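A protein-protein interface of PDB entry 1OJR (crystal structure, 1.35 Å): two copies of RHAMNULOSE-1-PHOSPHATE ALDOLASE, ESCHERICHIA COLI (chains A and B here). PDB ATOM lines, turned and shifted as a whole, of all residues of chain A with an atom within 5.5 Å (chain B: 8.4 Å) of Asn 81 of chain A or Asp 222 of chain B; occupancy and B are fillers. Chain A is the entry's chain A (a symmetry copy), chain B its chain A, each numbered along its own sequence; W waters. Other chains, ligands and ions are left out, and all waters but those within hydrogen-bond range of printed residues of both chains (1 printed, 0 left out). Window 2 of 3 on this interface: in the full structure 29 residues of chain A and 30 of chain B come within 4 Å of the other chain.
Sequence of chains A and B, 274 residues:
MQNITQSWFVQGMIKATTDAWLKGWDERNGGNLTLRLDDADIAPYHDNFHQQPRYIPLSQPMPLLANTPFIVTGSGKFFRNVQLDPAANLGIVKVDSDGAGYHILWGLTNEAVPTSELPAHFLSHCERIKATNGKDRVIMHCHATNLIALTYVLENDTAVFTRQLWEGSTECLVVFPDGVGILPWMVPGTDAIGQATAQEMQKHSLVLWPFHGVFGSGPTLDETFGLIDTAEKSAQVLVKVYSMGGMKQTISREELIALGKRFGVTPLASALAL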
ATOM      1  N   PHE A  78      17.164 -19.743 -19.901  1.00  0.00           N
ATOM      2  CA  PHE A  78      17.258 -18.849 -21.044  1.00  0.00           C
ATOM      3  C   PHE A  78      16.903 -19.581 -22.336  1.00  0.00           C
ATOM      4  O   PHE A  78      17.481 -20.630 -22.628  1.00  0.00           O
ATOM      5  CB  PHE A  78      18.705 -18.375 -21.231  1.00  0.00           C
ATOM      6  CG  PHE A  78      19.207 -17.364 -20.226  1.00  0.00           C
ATOM      7  CD1 PHE A  78      18.613 -17.151 -18.997  1.00  0.00           C
ATOM      8  CD2 PHE A  78      20.319 -16.616 -20.548  1.00  0.00           C
ATOM      9  CE1 PHE A  78      19.140 -16.213 -18.121  1.00  0.00           C
ATOM     10  CE2 PHE A  78      20.839 -15.692 -19.684  1.00  0.00           C
ATOM     11  CZ  PHE A  78      20.265 -15.499 -18.470  1.00  0.00           C
ATOM     12  N   PHE A  79      16.016 -19.006 -23.144  1.00  0.00           N
ATOM     13  CA  PHE A  79      15.712 -19.594 -24.444  1.00  0.00           C
ATOM     14  C   PHE A  79      16.996 -19.827 -25.250  1.00  0.00           C
ATOM     15  O   PHE A  79      17.118 -20.811 -25.984  1.00  0.00           O
ATOM     16  CB  PHE A  79      14.792 -18.685 -25.273  1.00  0.00           C
ATOM     17  CG  PHE A  79      13.308 -18.875 -25.016  1.00  0.00           C
ATOM     18  CD1 PHE A  79      12.823 -19.350 -23.804  1.00  0.00           C
ATOM     19  CD2 PHE A  79      12.397 -18.549 -25.999  1.00  0.00           C
ATOM     20  CE1 PHE A  79      11.467 -19.499 -23.596  1.00  0.00           C
ATOM     21  CE2 PHE A  79      11.047 -18.709 -25.796  1.00  0.00           C
ATOM     22  CZ  PHE A  79      10.579 -19.184 -24.592  1.00  0.00           C
ATOM     23  N   ARG A  80      17.955 -18.910 -25.136  1.00  0.00           N
ATOM     24  CA  ARG A  80      19.201 -19.005 -25.892  1.00  0.00           C
ATOM     25  C   ARG A  80      19.974 -20.290 -25.616  1.00  0.00           C
ATOM     26  O   ARG A  80      20.706 -20.780 -26.480  1.00  0.00           O
ATOM     27  CB  ARG A  80      20.080 -17.811 -25.547  1.00  0.00           C
ATOM     28  CG  ARG A  80      21.310 -17.669 -26.410  1.00  0.00           C
ATOM     29  CD  ARG A  80      22.574 -18.258 -25.821  1.00  0.00           C
ATOM     30  NE  ARG A  80      23.668 -18.163 -26.786  1.00  0.00           N
ATOM     31  CZ  ARG A  80      23.925 -19.051 -27.734  1.00  0.00           C
ATOM     32  NH1 ARG A  80      23.228 -20.169 -27.849  1.00  0.00           N
ATOM     33  NH2 ARG A  80      24.924 -18.836 -28.567  1.00  0.00           N
ATOM     34  N   ASN A  81      19.801 -20.834 -24.417  1.00  0.00           N
ATOM     35  CA  ASN A  81      20.562 -21.998 -23.978  1.00  0.00           C
ATOM     36  C   ASN A  81      19.900 -23.348 -24.238  1.00  0.00           C
ATOM     37  O   ASN A  81      20.541 -24.397 -24.086  1.00  0.00           O
ATOM     38  CB  ASN A  81      20.854 -21.897 -22.480  1.00  0.00           C
ATOM     39  CG  ASN A  81      21.868 -20.827 -22.154  1.00  0.00           C
ATOM     40  OD1 ASN A  81      22.661 -20.418 -23.015  1.00  0.00           O
ATOM     41  ND2 ASN A  81      21.859 -20.371 -20.905  1.00  0.00           N
ATOM     42  N   VAL A  82      18.629 -23.344 -24.623  1.00  0.00           N
ATOM     43  CA  VAL A  82      17.916 -24.603 -24.825  1.00  0.00           C
ATOM     44  C   VAL A  82      18.663 -25.517 -25.806  1.00  0.00           C
ATOM     45  O   VAL A  82      18.804 -26.713 -25.570  1.00  0.00           O
ATOM     46  CB  VAL A  82      16.460 -24.348 -25.272  1.00  0.00           C
ATOM     47  CG1 VAL A  82      15.762 -25.637 -25.653  1.00  0.00           C
ATOM     48  CG2 VAL A  82      15.691 -23.630 -24.157  1.00  0.00           C
ATOM     49  N   GLN A  83      19.151 -24.959 -26.904  1.00  0.00           N
ATOM     50  CA  GLN A  83      19.866 -25.741 -27.907  1.00  0.00           C
ATOM     51  C   GLN A  83      21.182 -26.317 -27.393  1.00  0.00           C
ATOM     52  O   GLN A  83      21.678 -27.310 -27.921  1.00  0.00           O
ATOM     53  CB  GLN A  83      20.155 -24.873 -29.126  1.00  0.00           C
ATOM     54  CG  GLN A  83      21.083 -23.715 -28.834  1.00  0.00           C
ATOM     55  CD  GLN A  83      21.156 -22.746 -29.981  1.00  0.00           C
ATOM     56  OE1 GLN A  83      21.428 -23.147 -31.126  1.00  0.00           O
ATOM     57  NE2 GLN A  83      20.908 -21.468 -29.696  1.00  0.00           N
ATOM     58  N   LEU A  84      21.768 -25.662 -26.399  1.00  0.00           N
ATOM     59  CA  LEU A  84      23.046 -26.091 -25.853  1.00  0.00           C
ATOM     60  C   LEU A  84      22.918 -27.231 -24.859  1.00  0.00           C
ATOM     61  O   LEU A  84      23.840 -28.017 -24.705  1.00  0.00           O
ATOM     62  CB  LEU A  84      23.746 -24.920 -25.165  1.00  0.00           C
ATOM     63  CG  LEU A  84      23.973 -23.666 -26.001  1.00  0.00           C
ATOM     64  CD1 LEU A  84      24.665 -22.575 -25.198  1.00  0.00           C
ATOM     65  CD2 LEU A  84      24.771 -23.980 -27.249  1.00  0.00           C
ATOM     66  N   ASP A  85      21.794 -27.281 -24.150  1.00  0.00           N
ATOM     67  CA  ASP A  85      21.571 -28.301 -23.135  1.00  0.00           C
ATOM     68  C   ASP A  85      20.077 -28.470 -22.916  1.00  0.00           C
ATOM     69  O   ASP A  85      19.505 -27.935 -21.963  1.00  0.00           O
ATOM     70  CB  ASP A  85      22.267 -27.904 -21.833  1.00  0.00           C
ATOM     71  CG  ASP A  85      22.359 -29.047 -20.855  1.00  0.00           C
ATOM     72  OD1 ASP A  85      23.206 -28.984 -19.929  1.00  0.00           O
ATOM     73  OD2 ASP A  85      21.615 -30.048 -20.939  1.00  0.00           O
ATOM     74  N   PRO A  86      19.438 -29.218 -23.806  1.00  0.00           N
ATOM     75  CA  PRO A  86      17.995 -29.428 -23.721  1.00  0.00           C
ATOM     76  C   PRO A  86      17.537 -29.980 -22.372  1.00  0.00           C
ATOM     77  O   PRO A  86      16.568 -29.476 -21.827  1.00  0.00           O
ATOM     78  CB  PRO A  86      17.716 -30.405 -24.865  1.00  0.00           C
ATOM     79  CG  PRO A  86      18.832 -30.177 -25.836  1.00  0.00           C
ATOM     80  CD  PRO A  86      20.027 -29.848 -24.999  1.00  0.00           C
ATOM     81  N   ASN A  89      17.368 -27.301 -19.584  1.00  0.00           N
ATOM     82  CA  ASN A  89      16.483 -26.167 -19.774  1.00  0.00           C
ATOM     83  C   ASN A  89      15.036 -26.502 -20.047  1.00  0.00           C
ATOM     84  O   ASN A  89      14.174 -25.623 -19.950  1.00  0.00           O
ATOM     85  CB  ASN A  89      17.061 -25.299 -20.888  1.00  0.00           C
ATOM     86  CG  ASN A  89      18.397 -24.710 -20.496  1.00  0.00           C
ATOM     87  OD1 ASN A  89      18.455 -23.862 -19.612  1.00  0.00           O
ATOM     88  ND2 ASN A  89      19.479 -25.198 -21.101  1.00  0.00           N
ATOM     89  N   TRP B   8      34.731 -24.803 -19.724  1.00  0.00           N
ATOM     90  CA  TRP B   8      33.498 -24.038 -19.600  1.00  0.00           C
ATOM     91  C   TRP B   8      33.746 -22.545 -19.692  1.00  0.00           C
ATOM     92  O   TRP B   8      32.919 -21.821 -20.244  1.00  0.00           O
ATOM     93  CB  TRP B   8      32.740 -24.370 -18.301  1.00  0.00           C
ATOM     94  CG  TRP B   8      33.367 -23.886 -17.022  1.00  0.00           C
ATOM     95  CD1 TRP B   8      34.126 -24.616 -16.153  1.00  0.00           C
ATOM     96  CD2 TRP B   8      33.261 -22.574 -16.452  1.00  0.00           C
ATOM     97  NE1 TRP B   8      34.513 -23.834 -15.092  1.00  0.00           N
ATOM     98  CE2 TRP B   8      33.994 -22.576 -15.249  1.00  0.00           C
ATOM     99  CE3 TRP B   8      32.636 -21.388 -16.846  1.00  0.00           C
ATOM    100  CZ2 TRP B   8      34.111 -21.449 -14.441  1.00  0.00           C
ATOM    101  CZ3 TRP B   8      32.749 -20.275 -16.043  1.00  0.00           C
ATOM    102  CH2 TRP B   8      33.484 -20.311 -14.856  1.00  0.00           C
ATOM    103  N   GLY B  12      32.521 -20.211 -22.564  1.00  0.00           N
ATOM    104  CA  GLY B  12      31.609 -19.176 -22.104  1.00  0.00           C
ATOM    105  C   GLY B  12      32.028 -17.807 -22.620  1.00  0.00           C
ATOM    106  O   GLY B  12      31.185 -17.000 -23.015  1.00  0.00           O
ATOM    107  N   LYS B  15      31.068 -17.682 -26.212  1.00  0.00           N
ATOM    108  CA  LYS B  15      29.633 -17.510 -26.393  1.00  0.00           C
ATOM    109  C   LYS B  15      29.189 -16.075 -26.153  1.00  0.00           C
ATOM    110  O   LYS B  15      28.419 -15.524 -26.936  1.00  0.00           O
ATOM    111  CB  LYS B  15      28.839 -18.447 -25.479  1.00  0.00           C
ATOM    112  CG  LYS B  15      27.346 -18.491 -25.805  1.00  0.00           C
ATOM    113  CD  LYS B  15      26.550 -19.372 -24.857  1.00  0.00           C
ATOM    114  CE  LYS B  15      25.830 -18.546 -23.818  1.00  0.00           C
ATOM    115  NZ  LYS B  15      25.167 -19.335 -22.734  1.00  0.00           N
ATOM    116  N   ALA B  16      29.667 -15.473 -25.068  1.00  0.00           N
ATOM    117  CA  ALA B  16      29.237 -14.130 -24.701  1.00  0.00           C
ATOM    118  C   ALA B  16      29.701 -13.095 -25.707  1.00  0.00           C
ATOM    119  O   ALA B  16      28.931 -12.221 -26.109  1.00  0.00           O
ATOM    120  CB  ALA B  16      29.733 -13.766 -23.312  1.00  0.00           C
ATOM    121  N   ASP B  19      27.835 -13.709 -29.057  1.00  0.00           N
ATOM    122  CA  ASP B  19      26.450 -13.268 -28.944  1.00  0.00           C
ATOM    123  C   ASP B  19      26.352 -11.740 -29.002  1.00  0.00           C
ATOM    124  O   ASP B  19      25.458 -11.195 -29.636  1.00  0.00           O
ATOM    125  CB  ASP B  19      25.812 -13.747 -27.640  1.00  0.00           C
ATOM    126  CG  ASP B  19      25.490 -15.222 -27.641  1.00  0.00           C
ATOM    127  OD1 ASP B  19      25.559 -15.887 -28.698  1.00  0.00           O
ATOM    128  OD2 ASP B  19      25.126 -15.789 -26.585  1.00  0.00           O
ATOM    129  N   LEU B  33      35.504  -7.724 -21.793  1.00  0.00           N
ATOM    130  CA  LEU B  33      34.864  -8.663 -20.894  1.00  0.00           C
ATOM    131  C   LEU B  33      35.901  -9.349 -20.020  1.00  0.00           C
ATOM    132  O   LEU B  33      36.918  -9.825 -20.511  1.00  0.00           O
ATOM    133  CB  LEU B  33      34.111  -9.699 -21.742  1.00  0.00           C
ATOM    134  CG  LEU B  33      33.383 -10.839 -21.031  1.00  0.00           C
ATOM    135  CD1 LEU B  33      32.276 -10.307 -20.129  1.00  0.00           C
ATOM    136  CD2 LEU B  33      32.847 -11.831 -22.060  1.00  0.00           C
ATOM    137  N   LEU B  35      36.210 -12.140 -16.550  1.00  0.00           N
ATOM    138  CA  LEU B  35      35.550 -13.125 -15.711  1.00  0.00           C
ATOM    139  C   LEU B  35      36.534 -13.628 -14.663  1.00  0.00           C
ATOM    140  O   LEU B  35      37.622 -14.111 -15.004  1.00  0.00           O
ATOM    141  CB  LEU B  35      35.086 -14.296 -16.577  1.00  0.00           C
ATOM    142  CG  LEU B  35      34.732 -15.617 -15.886  1.00  0.00           C
ATOM    143  CD1 LEU B  35      33.516 -15.454 -14.964  1.00  0.00           C
ATOM    144  CD2 LEU B  35      34.479 -16.684 -16.944  1.00  0.00           C
ATOM    145  N   VAL B 138      31.782 -11.207 -12.918  1.00  0.00           N
ATOM    146  CA  VAL B 138      31.913 -10.755 -14.293  1.00  0.00           C
ATOM    147  C   VAL B 138      31.718  -9.255 -14.411  1.00  0.00           C
ATOM    148  O   VAL B 138      30.818  -8.691 -13.782  1.00  0.00           O
ATOM    149  CB  VAL B 138      30.846 -11.425 -15.200  1.00  0.00           C
ATOM    150  CG1 VAL B 138      30.990 -10.965 -16.643  1.00  0.00           C
ATOM    151  CG2 VAL B 138      30.945 -12.929 -15.110  1.00  0.00           C
ATOM    152  N   MET B 140      31.239  -6.783 -17.748  1.00  0.00           N
ATOM    153  CA  MET B 140      31.078  -6.742 -19.191  1.00  0.00           C
ATOM    154  C   MET B 140      30.791  -5.325 -19.657  1.00  0.00           C
ATOM    155  O   MET B 140      29.924  -4.647 -19.099  1.00  0.00           O
ATOM    156  CB  MET B 140      29.934  -7.657 -19.622  1.00  0.00           C
ATOM    157  CG  MET B 140      29.650  -7.603 -21.108  1.00  0.00           C
ATOM    158  SD  MET B 140      28.396  -8.793 -21.590  1.00  0.00           S
ATOM    159  CE  MET B 140      28.111  -8.275 -23.316  1.00  0.00           C
ATOM    160  N   GLY B 218      27.772  -9.172 -12.731  1.00  0.00           N
ATOM    161  CA  GLY B 218      26.935 -10.281 -12.325  1.00  0.00           C
ATOM    162  C   GLY B 218      27.749 -11.489 -11.910  1.00  0.00           C
ATOM    163  O   GLY B 218      28.969 -11.504 -12.073  1.00  0.00           O
ATOM    164  N   PRO B 219      27.080 -12.496 -11.352  1.00  0.00           N
ATOM    165  CA  PRO B 219      27.751 -13.711 -10.870  1.00  0.00           C
ATOM    166  C   PRO B 219      28.245 -14.669 -11.950  1.00  0.00           C
ATOM    167  O   PRO B 219      29.195 -15.416 -11.698  1.00  0.00           O
ATOM    168  CB  PRO B 219      26.662 -14.395 -10.027  1.00  0.00           C
ATOM    169  CG  PRO B 219      25.662 -13.328  -9.732  1.00  0.00           C
ATOM    170  CD  PRO B 219      25.666 -12.453 -10.940  1.00  0.00           C
ATOM    171  N   THR B 220      27.608 -14.662 -13.116  1.00  0.00           N
ATOM    172  CA  THR B 220      28.009 -15.544 -14.211  1.00  0.00           C
ATOM    173  C   THR B 220      27.946 -14.785 -15.518  1.00  0.00           C
ATOM    174  O   THR B 220      27.334 -13.715 -15.603  1.00  0.00           O
ATOM    175  CB  THR B 220      27.086 -16.763 -14.345  1.00  0.00           C
ATOM    176  OG1 THR B 220      25.769 -16.326 -14.710  1.00  0.00           O
ATOM    177  CG2 THR B 220      26.944 -17.533 -13.035  1.00  0.00           C
ATOM    178  N   LEU B 221      28.567 -15.349 -16.546  1.00  0.00           N
ATOM    179  CA  LEU B 221      28.514 -14.750 -17.876  1.00  0.00           C
ATOM    180  C   LEU B 221      27.071 -14.584 -18.345  1.00  0.00           C
ATOM    181  O   LEU B 221      26.685 -13.512 -18.791  1.00  0.00           O
ATOM    182  CB  LEU B 221      29.310 -15.578 -18.881  1.00  0.00           C
ATOM    183  CG  LEU B 221      30.829 -15.536 -18.695  1.00  0.00           C
ATOM    184  CD1 LEU B 221      31.475 -16.632 -19.489  1.00  0.00           C
ATOM    185  CD2 LEU B 221      31.384 -14.168 -19.107  1.00  0.00           C
ATOM    186  N   ASP B 222      26.267 -15.636 -18.241  1.00  0.00           N
ATOM    187  CA  ASP B 222      24.883 -15.544 -18.685  1.00  0.00           C
ATOM    188  C   ASP B 222      24.094 -14.501 -17.911  1.00  0.00           C
ATOM    189  O   ASP B 222      23.301 -13.771 -18.487  1.00  0.00           O
ATOM    190  CB  ASP B 222      24.167 -16.897 -18.573  1.00  0.00           C
ATOM    191  CG  ASP B 222      24.409 -17.785 -19.752  1.00  0.00           C
ATOM    192  OD1 ASP B 222      24.079 -18.998 -19.659  1.00  0.00           O
ATOM    193  OD2 ASP B 222      24.909 -17.356 -20.820  1.00  0.00           O
ATOM    194  N   GLU B 223      24.264 -14.453 -16.595  1.00  0.00           N
ATOM    195  CA  GLU B 223      23.488 -13.495 -15.819  1.00  0.00           C
ATOM    196  C   GLU B 223      23.906 -12.062 -16.143  1.00  0.00           C
ATOM    197  O   GLU B 223      23.075 -11.158 -16.165  1.00  0.00           O
ATOM    198  CB  GLU B 223      23.641 -13.750 -14.319  1.00  0.00           C
ATOM    199  CG  GLU B 223      22.950 -15.003 -13.807  1.00  0.00           C
ATOM    200  CD  GLU B 223      23.348 -15.335 -12.380  1.00  0.00           C
ATOM    201  OE1 GLU B 223      22.566 -15.043 -11.452  1.00  0.00           O
ATOM    202  OE2 GLU B 223      24.451 -15.880 -12.183  1.00  0.00           O
ATOM    203  N   THR B 224      25.179 -11.855 -16.443  1.00  0.00           N
ATOM    204  CA  THR B 224      25.663 -10.515 -16.735  1.00  0.00           C
ATOM    205  C   THR B 224      25.258 -10.088 -18.147  1.00  0.00           C
ATOM    206  O   THR B 224      24.825  -8.957 -18.368  1.00  0.00           O
ATOM    207  CB  THR B 224      27.179 -10.453 -16.561  1.00  0.00           C
ATOM    208  OG1 THR B 224      27.534 -10.934 -15.256  1.00  0.00           O
ATOM    209  CG2 THR B 224      27.667  -9.013 -16.608  1.00  0.00           C
ATOM    210  N   PHE B 225      25.419 -10.996 -19.102  1.00  0.00           N
ATOM    211  CA  PHE B 225      24.951 -10.753 -20.458  1.00  0.00           C
ATOM    212  C   PHE B 225      23.446 -10.488 -20.422  1.00  0.00           C
ATOM    213  O   PHE B 225      22.949  -9.536 -21.022  1.00  0.00           O
ATOM    214  CB  PHE B 225      25.247 -11.959 -21.364  1.00  0.00           C
ATOM    215  CG  PHE B 225      24.876 -11.727 -22.799  1.00  0.00           C
ATOM    216  CD1 PHE B 225      25.842 -11.388 -23.730  1.00  0.00           C
ATOM    217  CD2 PHE B 225      23.561 -11.819 -23.207  1.00  0.00           C
ATOM    218  CE1 PHE B 225      25.495 -11.148 -25.039  1.00  0.00           C
ATOM    219  CE2 PHE B 225      23.220 -11.572 -24.504  1.00  0.00           C
ATOM    220  CZ  PHE B 225      24.178 -11.242 -25.428  1.00  0.00           C
ATOM    221  N   GLY B 226      22.717 -11.322 -19.684  1.00  0.00           N
ATOM    222  CA  GLY B 226      21.276 -11.182 -19.560  1.00  0.00           C
ATOM    223  C   GLY B 226      20.837  -9.874 -18.927  1.00  0.00           C
ATOM    224  O   GLY B 226      19.807  -9.324 -19.290  1.00  0.00           O
ATOM    225  N   LEU B 227      21.620  -9.383 -17.978  1.00  0.00           N
ATOM    226  CA  LEU B 227      21.369  -8.104 -17.341  1.00  0.00           C
ATOM    227  C   LEU B 227      21.441  -6.974 -18.377  1.00  0.00           C
ATOM    228  O   LEU B 227      20.548  -6.134 -18.493  1.00  0.00           O
ATOM    229  CB  LEU B 227      22.413  -7.897 -16.241  1.00  0.00           C
ATOM    230  CG  LEU B 227      22.529  -6.500 -15.631  1.00  0.00           C
ATOM    231  CD1 LEU B 227      21.279  -6.131 -14.865  1.00  0.00           C
ATOM    232  CD2 LEU B 227      23.761  -6.413 -14.738  1.00  0.00           C
ATOM    233  N   ILE B 228      22.529  -6.946 -19.126  1.00  0.00           N
ATOM    234  CA  ILE B 228      22.690  -5.950 -20.167  1.00  0.00           C
ATOM    235  C   ILE B 228      21.622  -6.101 -21.259  1.00  0.00           C
ATOM    236  O   ILE B 228      21.046  -5.113 -21.695  1.00  0.00           O
ATOM    237  CB  ILE B 228      24.093  -6.036 -20.761  1.00  0.00           C
ATOM    238  CG1 ILE B 228      25.119  -5.541 -19.734  1.00  0.00           C
ATOM    239  CG2 ILE B 228      24.185  -5.230 -22.046  1.00  0.00           C
ATOM    240  CD1 ILE B 228      26.558  -5.781 -20.116  1.00  0.00           C
ATOM    241  N   ASP B 229      21.359  -7.338 -21.682  1.00  0.00           N
ATOM    242  CA  ASP B 229      20.367  -7.615 -22.722  1.00  0.00           C
ATOM    243  C   ASP B 229      18.985  -7.134 -22.273  1.00  0.00           C
ATOM    244  O   ASP B 229      18.208  -6.603 -23.057  1.00  0.00           O
ATOM    245  CB  ASP B 229      20.365  -9.115 -23.008  1.00  0.00           C
ATOM    246  CG  ASP B 229      19.813  -9.487 -24.375  1.00  0.00           C
ATOM    247  OD1 ASP B 229      19.766  -8.644 -25.306  1.00  0.00           O
ATOM    248  OD2 ASP B 229      19.419 -10.654 -24.584  1.00  0.00           O
ATOM    249  N   THR B 230      18.686  -7.292 -20.986  1.00  0.00           N
ATOM    250  CA  THR B 230      17.410  -6.800 -20.452  1.00  0.00           C
ATOM    251  C   THR B 230      17.317  -5.268 -20.537  1.00  0.00           C
ATOM    252  O   THR B 230      16.318  -4.718 -21.010  1.00  0.00           O
ATOM    253  CB  THR B 230      17.231  -7.285 -19.001  1.00  0.00           C
ATOM    254  OG1 THR B 230      17.144  -8.712 -18.975  1.00  0.00           O
ATOM    255  CG2 THR B 230      15.929  -6.796 -18.435  1.00  0.00           C
HETATM  256  O   HOH W   1      27.551 -17.575 -29.804  1.00  0.00           O
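The guanidinium group of Arg 80 of chain A is in salt-bridge range of the side-chain carboxylate of Asp 19 of chain B (2.8 Å). The side-chain amino group of Lys 15 of chain B is in hydrogen-bond range of the side-chain amide oxygen of Asn 81 of chain A, at 2.7 Å. The side-chain amide nitrogen (ND2) of Asn 81 of chain A is in hydrogen-bond range of the side-chain carboxylate (OD1) of Asp 222 of chain B (2.9 Å).
No position is printed for both chains. Of the 6 pairs that touch across the chains among the printed residues, none has its exchanged pair printed and touching as well.
O of Asp 222 of chain B touches CE2 of Phe 78 of chain A (3.3 Å). Arg 80 of chain A touches Lys 15 of chain B. CD1 of Leu 84 of chain A touches CD of Lys 15 of chain B, at 3.7 Å.
Water W1 bridges OD1 of Asp 19 of chain B (2.8 Å) and NH2 of Arg 80 of chain A (3.2 Å).
The side-chain amino group (NZ) of Lys 15 of chain B lies within salt-bridge range of the side-chain carboxylate (OD2) of Asp 222 of chain B. O of Asn 81 of chain A is in hydrogen-bond range of ND2 of Asn 89 of chain A (3.3 Å). The guanidinium group (NH1) of Arg 80 of chain A lies close to the side-chain amide nitrogen (NE2) of Gln 83 of chain A.
Printed residues of chain B within 4 Å of Phe 78 of chain A: Asp 222. Of the printed residues of chain B, Arg 80 of chain A touches Lys 15 and Asp 19. Asn 81 of chain A touches just these residues of chain B: Lys 15 and Asp 222. Printed residues of chain B within 4 Å of Leu 84 of chain A: Lys 15 (3.7 Å). Of the printed residues of chain A, Asp 19 of chain B touches Arg 80. Met 140 of chain B touches none of the printed residues of chain A. Asp 222 of chain B touches two residues of chain A. The nearest residue of chain B that does not touch Asn 81 of chain A is Asp 19 of chain B (6.3 Å). The nearest printed residue of chain A that does not touch Asp 222 of chain B is Arg 80 of chain A (5.6 Å). The nearest printed residue of chain B that does not touch Leu 84 of chain A is Asp 222 of chain B (6.6 Å).
Of the 10 printed residues of chain A, 4 touch a printed residue of chain B. Among the printed residues, Asp or Glu carboxylates within 4 Å of a Lys or Arg side-chain nitrogen of the other chain: Arg 80 of chain A with Asp 19 of chain B.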
